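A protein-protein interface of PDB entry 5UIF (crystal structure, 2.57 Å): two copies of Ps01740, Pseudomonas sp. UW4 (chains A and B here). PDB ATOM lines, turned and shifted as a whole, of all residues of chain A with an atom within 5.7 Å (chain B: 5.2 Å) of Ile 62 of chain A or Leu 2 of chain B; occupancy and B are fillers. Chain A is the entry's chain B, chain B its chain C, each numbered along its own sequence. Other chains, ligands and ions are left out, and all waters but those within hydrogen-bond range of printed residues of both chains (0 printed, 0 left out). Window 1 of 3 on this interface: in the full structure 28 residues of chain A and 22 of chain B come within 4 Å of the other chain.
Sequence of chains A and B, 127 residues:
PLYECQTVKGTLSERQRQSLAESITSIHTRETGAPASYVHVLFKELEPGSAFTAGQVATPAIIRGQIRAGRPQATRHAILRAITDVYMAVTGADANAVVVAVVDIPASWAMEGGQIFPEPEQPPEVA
The backbone carbonyl oxygen (O) of Leu 2 of chain B is in hydrogen-bond range of the backbone NH (N) of Gln 66 of chain B (2.8 Å).
O of Thr 7 of chain A is in hydrogen-bond range of N of Leu 46 of chain A (2.7 Å).
The backbone NH (N) of His 40 of chain B is in hydrogen-bond range of the backbone carbonyl oxygen (O) of Pro 1 of chain B, at 3.1 Å.
O of Tyr 3 of chain B sits at hydrogen-bond distance from N of Leu 42 of chain B, 2.7 Å away.
The backbone NH (N) of Ile 63 of chain A is in hydrogen-bond range of the backbone carbonyl oxygen (O) of Val 99 of chain A, 2.9 Å away.
O of Ala 61 of chain A is in hydrogen-bond range of N of Val 99 of chain A.
Hydrophobic or aromatic side chains of chain B that line the printed part of chain A: Leu 2, His 40 and Leu 42.
Of the 12 printed residues of chain A, 6 touch a printed residue of chain B.
Printed residues of chain A that touch a printed residue of chain B: Gln 6, Leu 46, Pro 60, Ile 62, Arg 64 and Val 99.
Along chain A the printed residues that touch a printed residue of chain B span positions 6 to 99.
Among the printed residues, 9 pairs touch across the chains.
Among the printed residues, pairs that only touch across the chains: Gln 6 of chain A with Leu 42 of chain B, Leu 46 of chain A with Leu 42 of chain B, Pro 60 of chain A with His 40 of chain B, Ile 62 of chain A with Leu 2 of chain B, Ile 62 of chain A with Leu 42 of chain B, Arg 64 of chain A with Gln 66 of chain B and Val 99 of chain A with His 40 of chain B.
Arg 64 of chain A touches Glu 4 of chain B, but with the chains exchanged Glu 4 of chain A does not touch Arg 64 of chain B (7.3 Å).
Positions printed for both chains: 4 and 64.
Of the 9 pairs that touch across the chains among the printed residues, none has its exchanged pair printed and touching as well.
Thr 7 of chain A touches none of the printed residues of chain B.
Of the printed residues of chain B, Leu 46 of chain A touches Leu 42 (3.7 Å).
Of the printed residues of chain B, Pro 60 of chain A touches His 40.
Of chain B, only Leu 2 (3.7 Å) and Leu 42 (3.8 Å) come within 4 Å of Ile 62 of chain A.
Of chain A, only Ile 62 comes within 4 Å of Leu 2 of chain B.
Of the printed residues of chain A, Glu 4 of chain B touches Gln 6 (3.3 Å) and Arg 64 (2.5 Å).
Val 41 of chain B touches none of the printed residues of chain A.
The nearest residue of chain B that does not touch Ile 62 of chain A is His 40 of chain B (5.1 Å).
The nearest printed residue of chain A that does not touch Gln 66 of chain B is Ile 62 of chain A (6.0 Å).
The guanidinium group of Arg 64 of chain A is in salt-bridge range of the side-chain carboxylate of Glu 4 of chain B (2.5 Å).
OE1 of Gln 6 of chain A lies close to OE1 of Glu 4 of chain B (3.3 Å).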
ATOM      1  N   GLU A   4     -26.672  -5.713  22.893  1.00  0.00           N
ATOM      2  CA  GLU A   4     -25.355  -6.263  23.186  1.00  0.00           C
ATOM      3  C   GLU A   4     -24.288  -5.179  23.124  1.00  0.00           C
ATOM      4  O   GLU A   4     -24.246  -4.393  22.179  1.00  0.00           O
ATOM      5  CB  GLU A   4     -25.011  -7.389  22.211  1.00  0.00           C
ATOM      6  CG  GLU A   4     -25.974  -8.560  22.243  1.00  0.00           C
ATOM      7  CD  GLU A   4     -25.691  -9.571  21.151  1.00  0.00           C
ATOM      8  OE1 GLU A   4     -24.821 -10.444  21.357  1.00  0.00           O
ATOM      9  OE2 GLU A   4     -26.334  -9.487  20.085  1.00  0.00           O
ATOM     10  N   CYS A   5     -23.427  -5.144  24.134  1.00  0.00           N
ATOM     11  CA  CYS A   5     -22.352  -4.163  24.185  1.00  0.00           C
ATOM     12  C   CYS A   5     -20.982  -4.838  24.164  1.00  0.00           C
ATOM     13  O   CYS A   5     -20.618  -5.555  25.096  1.00  0.00           O
ATOM     14  CB  CYS A   5     -22.487  -3.286  25.429  1.00  0.00           C
ATOM     15  SG  CYS A   5     -21.234  -1.993  25.563  1.00  0.00           S
ATOM     16  N   GLN A   6     -20.228  -4.606  23.093  1.00  0.00           N
ATOM     17  CA  GLN A   6     -18.890  -5.173  22.957  1.00  0.00           C
ATOM     18  C   GLN A   6     -17.812  -4.127  23.203  1.00  0.00           C
ATOM     19  O   GLN A   6     -17.770  -3.094  22.536  1.00  0.00           O
ATOM     20  CB  GLN A   6     -18.701  -5.788  21.570  1.00  0.00           C
ATOM     21  CG  GLN A   6     -19.393  -7.122  21.374  1.00  0.00           C
ATOM     22  CD  GLN A   6     -19.040  -7.760  20.046  1.00  0.00           C
ATOM     23  OE1 GLN A   6     -18.502  -8.865  19.998  1.00  0.00           O
ATOM     24  NE2 GLN A   6     -19.340  -7.061  18.957  1.00  0.00           N
ATOM     25  N   THR A   7     -16.943  -4.403  24.172  1.00  0.00           N
ATOM     26  CA  THR A   7     -15.809  -3.537  24.473  1.00  0.00           C
ATOM     27  C   THR A   7     -14.575  -4.376  24.780  1.00  0.00           C
ATOM     28  O   THR A   7     -14.666  -5.592  24.946  1.00  0.00           O
ATOM     29  CB  THR A   7     -16.090  -2.604  25.674  1.00  0.00           C
ATOM     30  OG1 THR A   7     -16.440  -3.388  26.822  1.00  0.00           O
ATOM     31  CG2 THR A   7     -17.221  -1.633  25.366  1.00  0.00           C
ATOM     32  N   LEU A  46     -13.836  -8.150  24.984  1.00  0.00           N
ATOM     33  CA  LEU A  46     -12.830  -8.658  24.064  1.00  0.00           C
ATOM     34  C   LEU A  46     -11.445  -8.572  24.695  1.00  0.00           C
ATOM     35  O   LEU A  46     -11.125  -7.593  25.369  1.00  0.00           O
ATOM     36  CB  LEU A  46     -12.857  -7.875  22.751  1.00  0.00           C
ATOM     37  CG  LEU A  46     -14.159  -7.917  21.950  1.00  0.00           C
ATOM     38  CD1 LEU A  46     -14.251  -6.709  21.037  1.00  0.00           C
ATOM     39  CD2 LEU A  46     -14.249  -9.205  21.147  1.00  0.00           C
ATOM     40  N   PRO A  60     -12.395   0.082  20.302  1.00  0.00           N
ATOM     41  CA  PRO A  60     -13.708   0.539  19.841  1.00  0.00           C
ATOM     42  C   PRO A  60     -14.822   0.043  20.754  1.00  0.00           C
ATOM     43  O   PRO A  60     -14.588  -0.827  21.593  1.00  0.00           O
ATOM     44  CB  PRO A  60     -13.821  -0.080  18.448  1.00  0.00           C
ATOM     45  CG  PRO A  60     -13.031  -1.336  18.551  1.00  0.00           C
ATOM     46  CD  PRO A  60     -11.881  -1.029  19.479  1.00  0.00           C
ATOM     47  N   ALA A  61     -16.019   0.595  20.591  1.00  0.00           N
ATOM     48  CA  ALA A  61     -17.167   0.177  21.383  1.00  0.00           C
ATOM     49  C   ALA A  61     -18.370  -0.061  20.482  1.00  0.00           C
ATOM     50  O   ALA A  61     -18.838   0.854  19.805  1.00  0.00           O
ATOM     51  CB  ALA A  61     -17.489   1.213  22.443  1.00  0.00           C
ATOM     52  N   ILE A  62     -18.865  -1.292  20.474  1.00  0.00           N
ATOM     53  CA  ILE A  62     -19.979  -1.651  19.606  1.00  0.00           C
ATOM     54  C   ILE A  62     -21.220  -2.025  20.407  1.00  0.00           C
ATOM     55  O   ILE A  62     -21.229  -3.018  21.134  1.00  0.00           O
ATOM     56  CB  ILE A  62     -19.616  -2.820  18.669  1.00  0.00           C
ATOM     57  CG1 ILE A  62     -18.492  -2.413  17.712  1.00  0.00           C
ATOM     58  CG2 ILE A  62     -20.834  -3.264  17.880  1.00  0.00           C
ATOM     59  CD1 ILE A  62     -17.103  -2.773  18.198  1.00  0.00           C
ATOM     60  N   ILE A  63     -22.263  -1.215  20.269  1.00  0.00           N
ATOM     61  CA  ILE A  63     -23.544  -1.502  20.898  1.00  0.00           C
ATOM     62  C   ILE A  63     -24.583  -1.820  19.830  1.00  0.00           C
ATOM     63  O   ILE A  63     -24.975  -0.949  19.054  1.00  0.00           O
ATOM     64  CB  ILE A  63     -24.036  -0.327  21.760  1.00  0.00           C
ATOM     65  CG1 ILE A  63     -23.000   0.021  22.832  1.00  0.00           C
ATOM     66  CG2 ILE A  63     -25.378  -0.659  22.394  1.00  0.00           C
ATOM     67  CD1 ILE A  63     -23.411   1.164  23.733  1.00  0.00           C
ATOM     68  N   ARG A  64     -25.021  -3.073  19.790  1.00  0.00           N
ATOM     69  CA  ARG A  64     -25.995  -3.506  18.796  1.00  0.00           C
ATOM     70  C   ARG A  64     -27.316  -3.890  19.450  1.00  0.00           C
ATOM     71  O   ARG A  64     -27.352  -4.688  20.386  1.00  0.00           O
ATOM     72  CB  ARG A  64     -25.443  -4.679  17.986  1.00  0.00           C
ATOM     73  CG  ARG A  64     -24.249  -4.316  17.119  1.00  0.00           C
ATOM     74  CD  ARG A  64     -23.669  -5.539  16.432  1.00  0.00           C
ATOM     75  NE  ARG A  64     -23.089  -6.475  17.389  1.00  0.00           N
ATOM     76  CZ  ARG A  64     -22.595  -7.665  17.062  1.00  0.00           C
ATOM     77  NH1 ARG A  64     -22.611  -8.066  15.798  1.00  0.00           N
ATOM     78  NH2 ARG A  64     -22.086  -8.453  17.998  1.00  0.00           N
ATOM     79  N   VAL A  99     -19.637   2.853  18.117  1.00  0.00           N
ATOM     80  CA  VAL A  99     -20.579   2.490  17.064  1.00  0.00           C
ATOM     81  C   VAL A  99     -21.856   1.892  17.648  1.00  0.00           C
ATOM     82  O   VAL A  99     -21.811   0.906  18.383  1.00  0.00           O
ATOM     83  CB  VAL A  99     -19.964   1.484  16.071  1.00  0.00           C
ATOM     84  CG1 VAL A  99     -20.987   1.088  15.017  1.00  0.00           C
ATOM     85  CG2 VAL A  99     -18.723   2.071  15.418  1.00  0.00           C
ATOM     86  N   VAL A 100     -22.993   2.497  17.316  1.00  0.00           N
ATOM     87  CA  VAL A 100     -24.285   2.014  17.792  1.00  0.00           C
ATOM     88  C   VAL A 100     -25.182   1.619  16.622  1.00  0.00           C
ATOM     89  O   VAL A 100     -25.318   2.367  15.654  1.00  0.00           O
ATOM     90  CB  VAL A 100     -25.007   3.076  18.648  1.00  0.00           C
ATOM     91  CG1 VAL A 100     -26.309   2.521  19.198  1.00  0.00           C
ATOM     92  CG2 VAL A 100     -24.107   3.546  19.781  1.00  0.00           C
ATOM     93  N   PRO B   1     -18.108  -0.209   9.162  1.00  0.00           N
ATOM     94  CA  PRO B   1     -18.206  -1.663   9.000  1.00  0.00           C
ATOM     95  C   PRO B   1     -17.618  -2.426  10.184  1.00  0.00           C
ATOM     96  O   PRO B   1     -16.661  -1.963  10.802  1.00  0.00           O
ATOM     97  CB  PRO B   1     -17.397  -1.926   7.731  1.00  0.00           C
ATOM     98  CG  PRO B   1     -16.410  -0.815   7.692  1.00  0.00           C
ATOM     99  CD  PRO B   1     -17.145   0.384   8.218  1.00  0.00           C
ATOM    100  N   LEU B   2     -18.188  -3.589  10.483  1.00  0.00           N
ATOM    101  CA  LEU B   2     -17.737  -4.397  11.609  1.00  0.00           C
ATOM    102  C   LEU B   2     -17.520  -5.851  11.202  1.00  0.00           C
ATOM    103  O   LEU B   2     -18.443  -6.516  10.735  1.00  0.00           O
ATOM    104  CB  LEU B   2     -18.747  -4.322  12.756  1.00  0.00           C
ATOM    105  CG  LEU B   2     -18.462  -5.217  13.963  1.00  0.00           C
ATOM    106  CD1 LEU B   2     -17.171  -4.796  14.652  1.00  0.00           C
ATOM    107  CD2 LEU B   2     -19.631  -5.197  14.936  1.00  0.00           C
ATOM    108  N   TYR B   3     -16.298  -6.339  11.388  1.00  0.00           N
ATOM    109  CA  TYR B   3     -15.972  -7.726  11.079  1.00  0.00           C
ATOM    110  C   TYR B   3     -15.607  -8.492  12.347  1.00  0.00           C
ATOM    111  O   TYR B   3     -14.731  -8.073  13.104  1.00  0.00           O
ATOM    112  CB  TYR B   3     -14.830  -7.799  10.064  1.00  0.00           C
ATOM    113  CG  TYR B   3     -15.187  -7.254   8.699  1.00  0.00           C
ATOM    114  CD1 TYR B   3     -15.002  -5.911   8.395  1.00  0.00           C
ATOM    115  CD2 TYR B   3     -15.711  -8.082   7.715  1.00  0.00           C
ATOM    116  CE1 TYR B   3     -15.329  -5.410   7.148  1.00  0.00           C
ATOM    117  CE2 TYR B   3     -16.041  -7.589   6.466  1.00  0.00           C
ATOM    118  CZ  TYR B   3     -15.847  -6.252   6.188  1.00  0.00           C
ATOM    119  OH  TYR B   3     -16.174  -5.758   4.947  1.00  0.00           O
ATOM    120  N   GLU B   4     -16.284  -9.614  12.574  1.00  0.00           N
ATOM    121  CA  GLU B   4     -16.048 -10.425  13.765  1.00  0.00           C
ATOM    122  C   GLU B   4     -15.576 -11.827  13.396  1.00  0.00           C
ATOM    123  O   GLU B   4     -16.232 -12.529  12.627  1.00  0.00           O
ATOM    124  CB  GLU B   4     -17.316 -10.514  14.617  1.00  0.00           C
ATOM    125  CG  GLU B   4     -17.915  -9.168  14.989  1.00  0.00           C
ATOM    126  CD  GLU B   4     -19.153  -9.304  15.854  1.00  0.00           C
ATOM    127  OE1 GLU B   4     -19.057  -9.917  16.939  1.00  0.00           O
ATOM    128  OE2 GLU B   4     -20.221  -8.802  15.448  1.00  0.00           O
ATOM    129  N   HIS B  40     -13.669  -1.885  11.654  1.00  0.00           N
ATOM    130  CA  HIS B  40     -13.334  -2.541  12.911  1.00  0.00           C
ATOM    131  C   HIS B  40     -13.296  -4.058  12.761  1.00  0.00           C
ATOM    132  O   HIS B  40     -14.222  -4.659  12.217  1.00  0.00           O
ATOM    133  CB  HIS B  40     -14.336  -2.156  14.003  1.00  0.00           C
ATOM    134  CG  HIS B  40     -14.485  -0.678  14.194  1.00  0.00           C
ATOM    135  ND1 HIS B  40     -13.599   0.070  14.940  1.00  0.00           N
ATOM    136  CD2 HIS B  40     -15.421   0.189  13.741  1.00  0.00           C
ATOM    137  CE1 HIS B  40     -13.982   1.334  14.935  1.00  0.00           C
ATOM    138  NE2 HIS B  40     -15.084   1.433  14.214  1.00  0.00           N
ATOM    139  N   VAL B  41     -12.221  -4.669  13.247  1.00  0.00           N
ATOM    140  CA  VAL B  41     -12.104  -6.121  13.252  1.00  0.00           C
ATOM    141  C   VAL B  41     -12.017  -6.640  14.684  1.00  0.00           C
ATOM    142  O   VAL B  41     -11.206  -6.163  15.479  1.00  0.00           O
ATOM    143  CB  VAL B  41     -10.874  -6.601  12.456  1.00  0.00           C
ATOM    144  CG1 VAL B  41     -10.813  -8.119  12.442  1.00  0.00           C
ATOM    145  CG2 VAL B  41     -10.912  -6.055  11.036  1.00  0.00           C
ATOM    146  N   LEU B  42     -12.859  -7.613  15.011  1.00  0.00           N
ATOM    147  CA  LEU B  42     -12.885  -8.183  16.353  1.00  0.00           C
ATOM    148  C   LEU B  42     -12.599  -9.680  16.320  1.00  0.00           C
ATOM    149  O   LEU B  42     -13.092 -10.396  15.447  1.00  0.00           O
ATOM    150  CB  LEU B  42     -14.237  -7.922  17.021  1.00  0.00           C
ATOM    151  CG  LEU B  42     -14.728  -6.473  17.043  1.00  0.00           C
ATOM    152  CD1 LEU B  42     -16.033  -6.365  17.818  1.00  0.00           C
ATOM    153  CD2 LEU B  42     -13.673  -5.544  17.626  1.00  0.00           C
ATOM    154  N   ARG B  64     -17.857 -12.917  10.301  1.00  0.00           N
ATOM    155  CA  ARG B  64     -19.061 -12.190   9.923  1.00  0.00           C
ATOM    156  C   ARG B  64     -18.788 -10.697   9.789  1.00  0.00           C
ATOM    157  O   ARG B  64     -18.143 -10.094  10.647  1.00  0.00           O
ATOM    158  CB  ARG B  64     -20.175 -12.435  10.945  1.00  0.00           C
ATOM    159  CG  ARG B  64     -21.311 -11.426  10.884  1.00  0.00           C
ATOM    160  CD  ARG B  64     -22.570 -11.961  11.547  1.00  0.00           C
ATOM    161  NE  ARG B  64     -23.768 -11.284  11.061  1.00  0.00           N
ATOM    162  CZ  ARG B  64     -24.602 -10.595  11.833  1.00  0.00           C
ATOM    163  NH1 ARG B  64     -24.375 -10.494  13.135  1.00  0.00           N
ATOM    164  NH2 ARG B  64     -25.667 -10.010  11.303  1.00  0.00           N
ATOM    165  N   GLY B  65     -19.281 -10.104   8.706  1.00  0.00           N
ATOM    166  CA  GLY B  65     -19.087  -8.688   8.464  1.00  0.00           C
ATOM    167  C   GLY B  65     -20.384  -7.933   8.246  1.00  0.00           C
ATOM    168  O   GLY B  65     -21.200  -8.310   7.408  1.00  0.00           O
ATOM    169  N   GLN B  66     -20.574  -6.862   9.010  1.00  0.00           N
ATOM    170  CA  GLN B  66     -21.720  -5.985   8.815  1.00  0.00           C
ATOM    171  C   GLN B  66     -21.308  -4.740   8.039  1.00  0.00           C
ATOM    172  O   GLN B  66     -20.505  -3.939   8.515  1.00  0.00           O
ATOM    173  CB  GLN B  66     -22.343  -5.590  10.157  1.00  0.00           C
ATOM    174  CG  GLN B  66     -23.147  -6.697  10.820  1.00  0.00           C
ATOM    175  CD  GLN B  66     -23.830  -6.238  12.092  1.00  0.00           C
ATOM    176  OE1 GLN B  66     -23.232  -5.546  12.917  1.00  0.00           O
ATOM    177  NE2 GLN B  66     -25.093  -6.617  12.255  1.00  0.00           N
